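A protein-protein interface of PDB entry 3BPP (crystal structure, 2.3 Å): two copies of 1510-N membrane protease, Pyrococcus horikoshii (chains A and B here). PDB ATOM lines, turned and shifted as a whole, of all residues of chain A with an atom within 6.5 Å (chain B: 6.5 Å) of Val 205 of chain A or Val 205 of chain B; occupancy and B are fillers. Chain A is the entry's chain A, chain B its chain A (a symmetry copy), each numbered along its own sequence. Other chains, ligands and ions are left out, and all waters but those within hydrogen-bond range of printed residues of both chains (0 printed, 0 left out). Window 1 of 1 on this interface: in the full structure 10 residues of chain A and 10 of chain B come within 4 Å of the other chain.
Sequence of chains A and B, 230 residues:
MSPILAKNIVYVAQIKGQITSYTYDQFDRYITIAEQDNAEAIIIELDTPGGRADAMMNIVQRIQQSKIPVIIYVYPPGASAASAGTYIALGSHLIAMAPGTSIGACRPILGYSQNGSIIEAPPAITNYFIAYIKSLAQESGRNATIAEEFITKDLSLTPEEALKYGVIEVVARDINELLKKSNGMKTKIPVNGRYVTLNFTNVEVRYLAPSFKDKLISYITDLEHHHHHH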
ATOM      1  N   ASN A   8      16.823  26.231 -21.946  1.00  0.00           N
ATOM      2  CA  ASN A   8      16.158  25.080 -21.326  1.00  0.00           C
ATOM      3  C   ASN A   8      17.167  23.964 -20.972  1.00  0.00           C
ATOM      4  O   ASN A   8      17.405  23.021 -21.728  1.00  0.00           O
ATOM      5  CB  ASN A   8      14.871  24.629 -22.060  1.00  0.00           C
ATOM      6  CG  ASN A   8      15.124  23.846 -23.334  1.00  0.00           C
ATOM      7  OD1 ASN A   8      16.203  23.900 -23.926  1.00  0.00           O
ATOM      8  ND2 ASN A   8      14.102  23.114 -23.771  1.00  0.00           N
ATOM      9  N   ILE A   9      17.778  24.141 -19.804  1.00  0.00           N
ATOM     10  CA  ILE A   9      18.819  23.279 -19.280  1.00  0.00           C
ATOM     11  C   ILE A   9      18.703  23.305 -17.749  1.00  0.00           C
ATOM     12  O   ILE A   9      18.832  24.363 -17.124  1.00  0.00           O
ATOM     13  CB  ILE A   9      20.224  23.700 -19.838  1.00  0.00           C
ATOM     14  CG1 ILE A   9      21.225  22.533 -19.842  1.00  0.00           C
ATOM     15  CG2 ILE A   9      20.762  24.957 -19.163  1.00  0.00           C
ATOM     16  CD1 ILE A   9      22.259  22.563 -18.762  1.00  0.00           C
ATOM     17  N   VAL A  10      18.381  22.159 -17.148  1.00  0.00           N
ATOM     18  CA  VAL A  10      18.234  22.081 -15.689  1.00  0.00           C
ATOM     19  C   VAL A  10      19.506  21.496 -15.122  1.00  0.00           C
ATOM     20  O   VAL A  10      20.079  20.599 -15.719  1.00  0.00           O
ATOM     21  CB  VAL A  10      17.045  21.230 -15.266  1.00  0.00           C
ATOM     22  CG1 VAL A  10      16.665  21.531 -13.813  1.00  0.00           C
ATOM     23  CG2 VAL A  10      15.869  21.545 -16.108  1.00  0.00           C
ATOM     24  N   TYR A  11      19.977  22.032 -14.002  1.00  0.00           N
ATOM     25  CA  TYR A  11      21.108  21.429 -13.315  1.00  0.00           C
ATOM     26  C   TYR A  11      20.633  20.576 -12.136  1.00  0.00           C
ATOM     27  O   TYR A  11      19.564  20.803 -11.598  1.00  0.00           O
ATOM     28  CB  TYR A  11      22.119  22.485 -12.888  1.00  0.00           C
ATOM     29  CG  TYR A  11      23.012  22.945 -14.026  1.00  0.00           C
ATOM     30  CD1 TYR A  11      24.304  22.455 -14.156  1.00  0.00           C
ATOM     31  CD2 TYR A  11      22.553  23.853 -14.980  1.00  0.00           C
ATOM     32  CE1 TYR A  11      25.123  22.865 -15.189  1.00  0.00           C
ATOM     33  CE2 TYR A  11      23.363  24.269 -16.029  1.00  0.00           C
ATOM     34  CZ  TYR A  11      24.648  23.776 -16.123  1.00  0.00           C
ATOM     35  OH  TYR A  11      25.467  24.184 -17.153  1.00  0.00           O
ATOM     36  N   VAL A  12      21.405  19.558 -11.777  1.00  0.00           N
ATOM     37  CA  VAL A  12      21.068  18.766 -10.624  1.00  0.00           C
ATOM     38  C   VAL A  12      22.324  18.583  -9.828  1.00  0.00           C
ATOM     39  O   VAL A  12      23.382  18.332 -10.397  1.00  0.00           O
ATOM     40  CB  VAL A  12      20.429  17.361 -10.969  1.00  0.00           C
ATOM     41  CG1 VAL A  12      20.285  16.556  -9.723  1.00  0.00           C
ATOM     42  CG2 VAL A  12      19.077  17.499 -11.687  1.00  0.00           C
ATOM     43  N   ILE A  43      17.973  21.906  -9.615  1.00  0.00           N
ATOM     44  CA  ILE A  43      17.388  21.008  -8.630  1.00  0.00           C
ATOM     45  C   ILE A  43      18.500  20.621  -7.671  1.00  0.00           C
ATOM     46  O   ILE A  43      19.549  20.186  -8.087  1.00  0.00           O
ATOM     47  CB  ILE A  43      16.726  19.742  -9.282  1.00  0.00           C
ATOM     48  CG1 ILE A  43      15.508  20.156 -10.133  1.00  0.00           C
ATOM     49  CG2 ILE A  43      16.303  18.702  -8.204  1.00  0.00           C
ATOM     50  CD1 ILE A  43      15.061  19.162 -11.185  1.00  0.00           C
ATOM     51  N   ILE A 175      14.182  12.280 -10.713  1.00  0.00           N
ATOM     52  CA  ILE A 175      14.373  13.514 -11.457  1.00  0.00           C
ATOM     53  C   ILE A 175      13.525  13.655 -12.739  1.00  0.00           C
ATOM     54  O   ILE A 175      13.084  14.743 -13.074  1.00  0.00           O
ATOM     55  CB  ILE A 175      15.866  13.697 -11.739  1.00  0.00           C
ATOM     56  CG1 ILE A 175      16.584  14.005 -10.424  1.00  0.00           C
ATOM     57  CG2 ILE A 175      16.133  14.750 -12.867  1.00  0.00           C
ATOM     58  CD1 ILE A 175      16.321  15.376  -9.925  1.00  0.00           C
ATOM     59  N   LEU A 179      10.607  16.403 -13.090  1.00  0.00           N
ATOM     60  CA  LEU A 179      10.626  17.291 -14.241  1.00  0.00           C
ATOM     61  C   LEU A 179       9.289  17.277 -14.996  1.00  0.00           C
ATOM     62  O   LEU A 179       8.849  18.307 -15.496  1.00  0.00           O
ATOM     63  CB  LEU A 179      11.809  16.959 -15.164  1.00  0.00           C
ATOM     64  CG  LEU A 179      13.199  17.481 -14.774  1.00  0.00           C
ATOM     65  CD1 LEU A 179      14.277  16.926 -15.673  1.00  0.00           C
ATOM     66  CD2 LEU A 179      13.276  18.988 -14.788  1.00  0.00           C
ATOM     67  N   VAL A 203      13.771  19.793 -22.067  1.00  0.00           N
ATOM     68  CA  VAL A 203      14.889  20.147 -21.197  1.00  0.00           C
ATOM     69  C   VAL A 203      15.989  19.112 -21.146  1.00  0.00           C
ATOM     70  O   VAL A 203      15.709  17.922 -21.065  1.00  0.00           O
ATOM     71  CB  VAL A 203      14.419  20.595 -19.801  1.00  0.00           C
ATOM     72  CG1 VAL A 203      14.272  19.408 -18.832  1.00  0.00           C
ATOM     73  CG2 VAL A 203      15.367  21.644 -19.267  1.00  0.00           C
ATOM     74  N   GLU A 204      17.231  19.590 -21.246  1.00  0.00           N
ATOM     75  CA  GLU A 204      18.435  18.790 -21.052  1.00  0.00           C
ATOM     76  C   GLU A 204      18.911  18.954 -19.619  1.00  0.00           C
ATOM     77  O   GLU A 204      18.919  20.058 -19.085  1.00  0.00           O
ATOM     78  CB  GLU A 204      19.541  19.216 -22.015  1.00  0.00           C
ATOM     79  CG  GLU A 204      19.119  19.146 -23.489  1.00  0.00           C
ATOM     80  CD  GLU A 204      20.199  19.616 -24.447  1.00  0.00           C
ATOM     81  OE1 GLU A 204      21.169  18.851 -24.686  1.00  0.00           O
ATOM     82  OE2 GLU A 204      20.064  20.748 -24.971  1.00  0.00           O
ATOM     83  N   VAL A 205      19.299  17.842 -19.004  1.00  0.00           N
ATOM     84  CA  VAL A 205      19.701  17.801 -17.612  1.00  0.00           C
ATOM     85  C   VAL A 205      21.202  17.661 -17.528  1.00  0.00           C
ATOM     86  O   VAL A 205      21.803  16.840 -18.233  1.00  0.00           O
ATOM     87  CB  VAL A 205      18.983  16.670 -16.865  1.00  0.00           C
ATOM     88  CG1 VAL A 205      19.316  16.659 -15.358  1.00  0.00           C
ATOM     89  CG2 VAL A 205      17.505  16.816 -17.053  1.00  0.00           C
ATOM     90  N   ARG A 206      21.818  18.504 -16.700  1.00  0.00           N
ATOM     91  CA  ARG A 206      23.208  18.343 -16.375  1.00  0.00           C
ATOM     92  C   ARG A 206      23.315  18.038 -14.897  1.00  0.00           C
ATOM     93  O   ARG A 206      22.719  18.735 -14.078  1.00  0.00           O
ATOM     94  CB  ARG A 206      24.036  19.572 -16.769  1.00  0.00           C
ATOM     95  CG  ARG A 206      24.414  19.589 -18.248  1.00  0.00           C
ATOM     96  CD  ARG A 206      25.538  20.582 -18.557  1.00  0.00           C
ATOM     97  NE  ARG A 206      25.433  21.099 -19.929  1.00  0.00           N
ATOM     98  CZ  ARG A 206      26.132  22.123 -20.425  1.00  0.00           C
ATOM     99  NH1 ARG A 206      25.942  22.503 -21.685  1.00  0.00           N
ATOM    100  NH2 ARG A 206      27.014  22.769 -19.672  1.00  0.00           N
ATOM    101  N   TYR A 207      24.076  16.985 -14.588  1.00  0.00           N
ATOM    102  CA  TYR A 207      24.345  16.539 -13.234  1.00  0.00           C
ATOM    103  C   TYR A 207      25.687  16.967 -12.773  1.00  0.00           C
ATOM    104  O   TYR A 207      26.697  16.627 -13.391  1.00  0.00           O
ATOM    105  CB  TYR A 207      24.299  15.022 -13.127  1.00  0.00           C
ATOM    106  CG  TYR A 207      22.919  14.452 -13.289  1.00  0.00           C
ATOM    107  CD1 TYR A 207      22.018  14.425 -12.207  1.00  0.00           C
ATOM    108  CD2 TYR A 207      22.492  13.951 -14.523  1.00  0.00           C
ATOM    109  CE1 TYR A 207      20.727  13.914 -12.361  1.00  0.00           C
ATOM    110  CE2 TYR A 207      21.191  13.416 -14.692  1.00  0.00           C
ATOM    111  CZ  TYR A 207      20.314  13.412 -13.608  1.00  0.00           C
ATOM    112  OH  TYR A 207      19.050  12.881 -13.762  1.00  0.00           O
ATOM    113  N   ASN B   8      27.857  14.279 -26.997  1.00  0.00           N
ATOM    114  CA  ASN B   8      27.684  13.810 -25.617  1.00  0.00           C
ATOM    115  C   ASN B   8      26.293  14.189 -25.060  1.00  0.00           C
ATOM    116  O   ASN B   8      26.097  15.214 -24.404  1.00  0.00           O
ATOM    117  CB  ASN B   8      28.893  14.111 -24.697  1.00  0.00           C
ATOM    118  CG  ASN B   8      28.982  15.554 -24.238  1.00  0.00           C
ATOM    119  OD1 ASN B   8      28.401  16.462 -24.833  1.00  0.00           O
ATOM    120  ND2 ASN B   8      29.736  15.769 -23.163  1.00  0.00           N
ATOM    121  N   ILE B   9      25.330  13.332 -25.389  1.00  0.00           N
ATOM    122  CA  ILE B   9      23.930  13.500 -25.055  1.00  0.00           C
ATOM    123  C   ILE B   9      23.331  12.096 -24.885  1.00  0.00           C
ATOM    124  O   ILE B   9      23.333  11.291 -25.822  1.00  0.00           O
ATOM    125  CB  ILE B   9      23.205  14.395 -26.122  1.00  0.00           C
ATOM    126  CG1 ILE B   9      21.967  15.101 -25.550  1.00  0.00           C
ATOM    127  CG2 ILE B   9      22.928  13.641 -27.418  1.00  0.00           C
ATOM    128  CD1 ILE B   9      20.647  14.521 -25.950  1.00  0.00           C
ATOM    129  N   VAL B  10      22.891  11.771 -23.669  1.00  0.00           N
ATOM    130  CA  VAL B  10      22.313  10.448 -23.398  1.00  0.00           C
ATOM    131  C   VAL B  10      20.809  10.585 -23.410  1.00  0.00           C
ATOM    132  O   VAL B  10      20.287  11.580 -22.935  1.00  0.00           O
ATOM    133  CB  VAL B  10      22.764   9.875 -22.061  1.00  0.00           C
ATOM    134  CG1 VAL B  10      22.517   8.364 -22.021  1.00  0.00           C
ATOM    135  CG2 VAL B  10      24.218  10.094 -21.880  1.00  0.00           C
ATOM    136  N   TYR B  11      20.114   9.617 -23.998  1.00  0.00           N
ATOM    137  CA  TYR B  11      18.662   9.600 -23.920  1.00  0.00           C
ATOM    138  C   TYR B  11      18.190   8.624 -22.840  1.00  0.00           C
ATOM    139  O   TYR B  11      18.891   7.687 -22.501  1.00  0.00           O
ATOM    140  CB  TYR B  11      18.041   9.297 -25.277  1.00  0.00           C
ATOM    141  CG  TYR B  11      18.011  10.505 -26.197  1.00  0.00           C
ATOM    142  CD1 TYR B  11      16.845  11.237 -26.368  1.00  0.00           C
ATOM    143  CD2 TYR B  11      19.156  10.920 -26.878  1.00  0.00           C
ATOM    144  CE1 TYR B  11      16.809  12.338 -27.200  1.00  0.00           C
ATOM    145  CE2 TYR B  11      19.137  12.030 -27.713  1.00  0.00           C
ATOM    146  CZ  TYR B  11      17.958  12.730 -27.873  1.00  0.00           C
ATOM    147  OH  TYR B  11      17.920  13.827 -28.704  1.00  0.00           O
ATOM    148  N   VAL B  12      17.024   8.882 -22.260  1.00  0.00           N
ATOM    149  CA  VAL B  12      16.475   7.962 -21.298  1.00  0.00           C
ATOM    150  C   VAL B  12      15.028   7.776 -21.639  1.00  0.00           C
ATOM    151  O   VAL B  12      14.340   8.743 -21.953  1.00  0.00           O
ATOM    152  CB  VAL B  12      16.628   8.429 -19.796  1.00  0.00           C
ATOM    153  CG1 VAL B  12      15.875   7.503 -18.903  1.00  0.00           C
ATOM    154  CG2 VAL B  12      18.101   8.522 -19.364  1.00  0.00           C
ATOM    155  N   ILE B  43      19.677   5.031 -22.565  1.00  0.00           N
ATOM    156  CA  ILE B  43      19.366   4.198 -21.413  1.00  0.00           C
ATOM    157  C   ILE B  43      17.885   3.872 -21.492  1.00  0.00           C
ATOM    158  O   ILE B  43      17.067   4.753 -21.625  1.00  0.00           O
ATOM    159  CB  ILE B  43      19.730   4.888 -20.049  1.00  0.00           C
ATOM    160  CG1 ILE B  43      21.257   5.071 -19.936  1.00  0.00           C
ATOM    161  CG2 ILE B  43      19.193   4.073 -18.838  1.00  0.00           C
ATOM    162  CD1 ILE B  43      21.731   6.118 -18.949  1.00  0.00           C
ATOM    163  N   ILE B 175      19.673   7.330 -12.418  1.00  0.00           N
ATOM    164  CA  ILE B 175      20.319   7.708 -13.666  1.00  0.00           C
ATOM    165  C   ILE B 175      21.642   8.487 -13.519  1.00  0.00           C
ATOM    166  O   ILE B 175      22.555   8.311 -14.310  1.00  0.00           O
ATOM    167  CB  ILE B 175      19.309   8.459 -14.538  1.00  0.00           C
ATOM    168  CG1 ILE B 175      18.242   7.475 -15.017  1.00  0.00           C
ATOM    169  CG2 ILE B 175      20.000   9.256 -15.694  1.00  0.00           C
ATOM    170  CD1 ILE B 175      18.733   6.547 -16.064  1.00  0.00           C
ATOM    171  N   LEU B 179      25.180   6.934 -14.646  1.00  0.00           N
ATOM    172  CA  LEU B 179      26.020   7.707 -15.545  1.00  0.00           C
ATOM    173  C   LEU B 179      27.442   7.883 -14.990  1.00  0.00           C
ATOM    174  O   LEU B 179      28.408   7.870 -15.745  1.00  0.00           O
ATOM    175  CB  LEU B 179      25.365   9.057 -15.878  1.00  0.00           C
ATOM    176  CG  LEU B 179      24.257   9.079 -16.942  1.00  0.00           C
ATOM    177  CD1 LEU B 179      23.591  10.431 -17.026  1.00  0.00           C
ATOM    178  CD2 LEU B 179      24.760   8.692 -18.311  1.00  0.00           C
ATOM    179  N   VAL B 203      27.991  15.082 -19.917  1.00  0.00           N
ATOM    180  CA  VAL B 203      26.821  14.627 -20.663  1.00  0.00           C
ATOM    181  C   VAL B 203      25.526  15.284 -20.247  1.00  0.00           C
ATOM    182  O   VAL B 203      25.274  15.447 -19.059  1.00  0.00           O
ATOM    183  CB  VAL B 203      26.728  13.091 -20.715  1.00  0.00           C
ATOM    184  CG1 VAL B 203      25.962  12.518 -19.509  1.00  0.00           C
ATOM    185  CG2 VAL B 203      26.107  12.673 -22.027  1.00  0.00           C
ATOM    186  N   GLU B 204      24.745  15.697 -21.248  1.00  0.00           N
ATOM    187  CA  GLU B 204      23.387  16.199 -21.074  1.00  0.00           C
ATOM    188  C   GLU B 204      22.407  15.062 -21.304  1.00  0.00           C
ATOM    189  O   GLU B 204      22.565  14.279 -22.235  1.00  0.00           O
ATOM    190  CB  GLU B 204      23.092  17.339 -22.045  1.00  0.00           C
ATOM    191  CG  GLU B 204      24.082  18.506 -21.925  1.00  0.00           C
ATOM    192  CD  GLU B 204      23.823  19.621 -22.924  1.00  0.00           C
ATOM    193  OE1 GLU B 204      22.864  20.409 -22.713  1.00  0.00           O
ATOM    194  OE2 GLU B 204      24.591  19.713 -23.911  1.00  0.00           O
ATOM    195  N   VAL B 205      21.400  14.978 -20.443  1.00  0.00           N
ATOM    196  CA  VAL B 205      20.421  13.908 -20.461  1.00  0.00           C
ATOM    197  C   VAL B 205      19.118  14.431 -21.018  1.00  0.00           C
ATOM    198  O   VAL B 205      18.651  15.509 -20.633  1.00  0.00           O
ATOM    199  CB  VAL B 205      20.240  13.303 -19.064  1.00  0.00           C
ATOM    200  CG1 VAL B 205      19.278  12.097 -19.069  1.00  0.00           C
ATOM    201  CG2 VAL B 205      21.574  12.879 -18.534  1.00  0.00           C
ATOM    202  N   ARG B 206      18.554  13.686 -21.969  1.00  0.00           N
ATOM    203  CA  ARG B 206      17.222  13.961 -22.434  1.00  0.00           C
ATOM    204  C   ARG B 206      16.345  12.780 -22.077  1.00  0.00           C
ATOM    205  O   ARG B 206      16.711  11.637 -22.345  1.00  0.00           O
ATOM    206  CB  ARG B 206      17.190  14.267 -23.937  1.00  0.00           C
ATOM    207  CG  ARG B 206      17.567  15.711 -24.259  1.00  0.00           C
ATOM    208  CD  ARG B 206      17.170  16.119 -25.681  1.00  0.00           C
ATOM    209  NE  ARG B 206      18.075  17.145 -26.217  1.00  0.00           N
ATOM    210  CZ  ARG B 206      18.116  17.553 -27.487  1.00  0.00           C
ATOM    211  NH1 ARG B 206      18.988  18.488 -27.852  1.00  0.00           N
ATOM    212  NH2 ARG B 206      17.298  17.031 -28.393  1.00  0.00           N
ATOM    213  N   TYR B 207      15.199  13.088 -21.466  1.00  0.00           N
ATOM    214  CA  TYR B 207      14.197  12.117 -21.071  1.00  0.00           C
ATOM    215  C   TYR B 207      13.059  12.086 -22.021  1.00  0.00           C
ATOM    216  O   TYR B 207      12.401  13.104 -22.240  1.00  0.00           O
ATOM    217  CB  TYR B 207      13.623  12.437 -19.699  1.00  0.00           C
ATOM    218  CG  TYR B 207      14.601  12.230 -18.577  1.00  0.00           C
ATOM    219  CD1 TYR B 207      14.822  10.947 -18.041  1.00  0.00           C
ATOM    220  CD2 TYR B 207      15.324  13.305 -18.051  1.00  0.00           C
ATOM    221  CE1 TYR B 207      15.747  10.750 -17.011  1.00  0.00           C
ATOM    222  CE2 TYR B 207      16.254  13.124 -16.998  1.00  0.00           C
ATOM    223  CZ  TYR B 207      16.465  11.842 -16.494  1.00  0.00           C
ATOM    224  OH  TYR B 207      17.359  11.660 -15.460  1.00  0.00           O
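The guanidinium group (NH1) of Arg 206 of chain B lies within salt-bridge range of the side-chain carboxylate (OE2) of Glu 204 of chain A (3.8 Å).
The backbone carbonyl oxygen of Val 205 of chain B is in hydrogen-bond range of the backbone NH of Val 205 of chain A (2.9 Å).
OE2 of Glu 204 of chain B lies within salt-bridge range of NH1 of Arg 206 of chain A, 3.8 Å away.
OH of Tyr 207 of chain B is in hydrogen-bond range of OH of Tyr 207 of chain A.
The side-chain carboxylate (OE1) of Glu 204 of chain A lies close to the side-chain carboxylate (OE1) of Glu 204 of chain B (3.0 Å).
The backbone carbonyl oxygen of Glu 204 of chain A sits at hydrogen-bond distance from the backbone NH of Val 10 of chain A, 2.9 Å away.
The backbone carbonyl oxygen (O) of Val 10 of chain A lies within hydrogen-bond range of the backbone NH (N) of Arg 206 of chain A (2.9 Å).
OH of Tyr 11 of chain A sits at hydrogen-bond distance from NH2 of Arg 206 of chain A, at 3.3 Å.
The backbone NH of Val 12 of chain A lies within hydrogen-bond range of the backbone carbonyl oxygen of Arg 206 of chain A, 2.8 Å away.
The side-chain hydroxyl (OH) of Tyr 11 of chain B lies within hydrogen-bond range of the guanidinium group (NH2) of Arg 206 of chain B (3.3 Å).
O of Arg 206 of chain B lies within hydrogen-bond range of N of Val 12 of chain B.
Of the 13 printed residues of chain B, 6 touch a printed residue of chain A.
Printed residues of chain B that touch a printed residue of chain A: Ile 9, Val 203, Glu 204, Val 205, Arg 206 and Tyr 207.
Hydrophobic or aromatic side chains of chain A that line the printed part of chain B: Ile 9, Val 205 and Tyr 207.
Among the printed residues, 13 pairs touch across the chains.
Ile 9 of chain A touches Glu 204 of chain B, and with the chains exchanged Glu 204 of chain A touches Ile 9 of chain B.
Glu 204 of chain A touches Val 205 of chain B, and with the chains exchanged Val 205 of chain A touches Glu 204 of chain B.
Glu 204 of chain A touches Arg 206 of chain B, and with the chains exchanged Arg 206 of chain A touches Glu 204 of chain B.
Val 205 of chain A touches its own counterpart, Val 205 of chain B.
13 positions are printed for both chains.
CG1 of Ile 9 of chain A touches OE1 of Glu 204 of chain B, 3.9 Å away.
Val 203 of chain A touches Val 205 of chain B (O to O, 3.8 Å).
CG1 of Ile 9 of chain B touches OE1 of Glu 204 of chain A (3.9 Å).
Glu 204 of chain A touches Val 205 of chain B (CA to O, 3.3 Å).
O of Val 203 of chain B touches O of Val 205 of chain A, 3.8 Å away.
Val 205 of chain A touches Glu 204 of chain B (O to CA, 3.3 Å).
Tyr 207 of chain B touches Val 205 of chain A (CE2 to CG2, 3.9 Å).
Tyr 207 of chain A touches Val 205 of chain B.
Of chain B, only Val 203, Glu 204, Val 205 and Tyr 207 come within 4 Å of Val 205 of chain A.
Of the printed residues of chain A, Val 203 of chain B touches Val 205.
Of chain A, only Val 203 (3.8 Å), Glu 204 (3.3 Å), Val 205 (2.9 Å) and Tyr 207 (3.9 Å) come within 4 Å of Val 205 of chain B.
Of the printed residues of chain A, Arg 206 of chain B touches Glu 204.
Of the printed residues of chain A, Tyr 207 of chain B touches Val 205 (3.9 Å) and Tyr 207 (2.7 Å).
The nearest residue of chain B that does not touch Val 205 of chain A is Arg 206 of chain B (5.2 Å).
The nearest printed residue of chain B that does not touch Ile 9 of chain A is Val 205 of chain B (7.5 Å).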
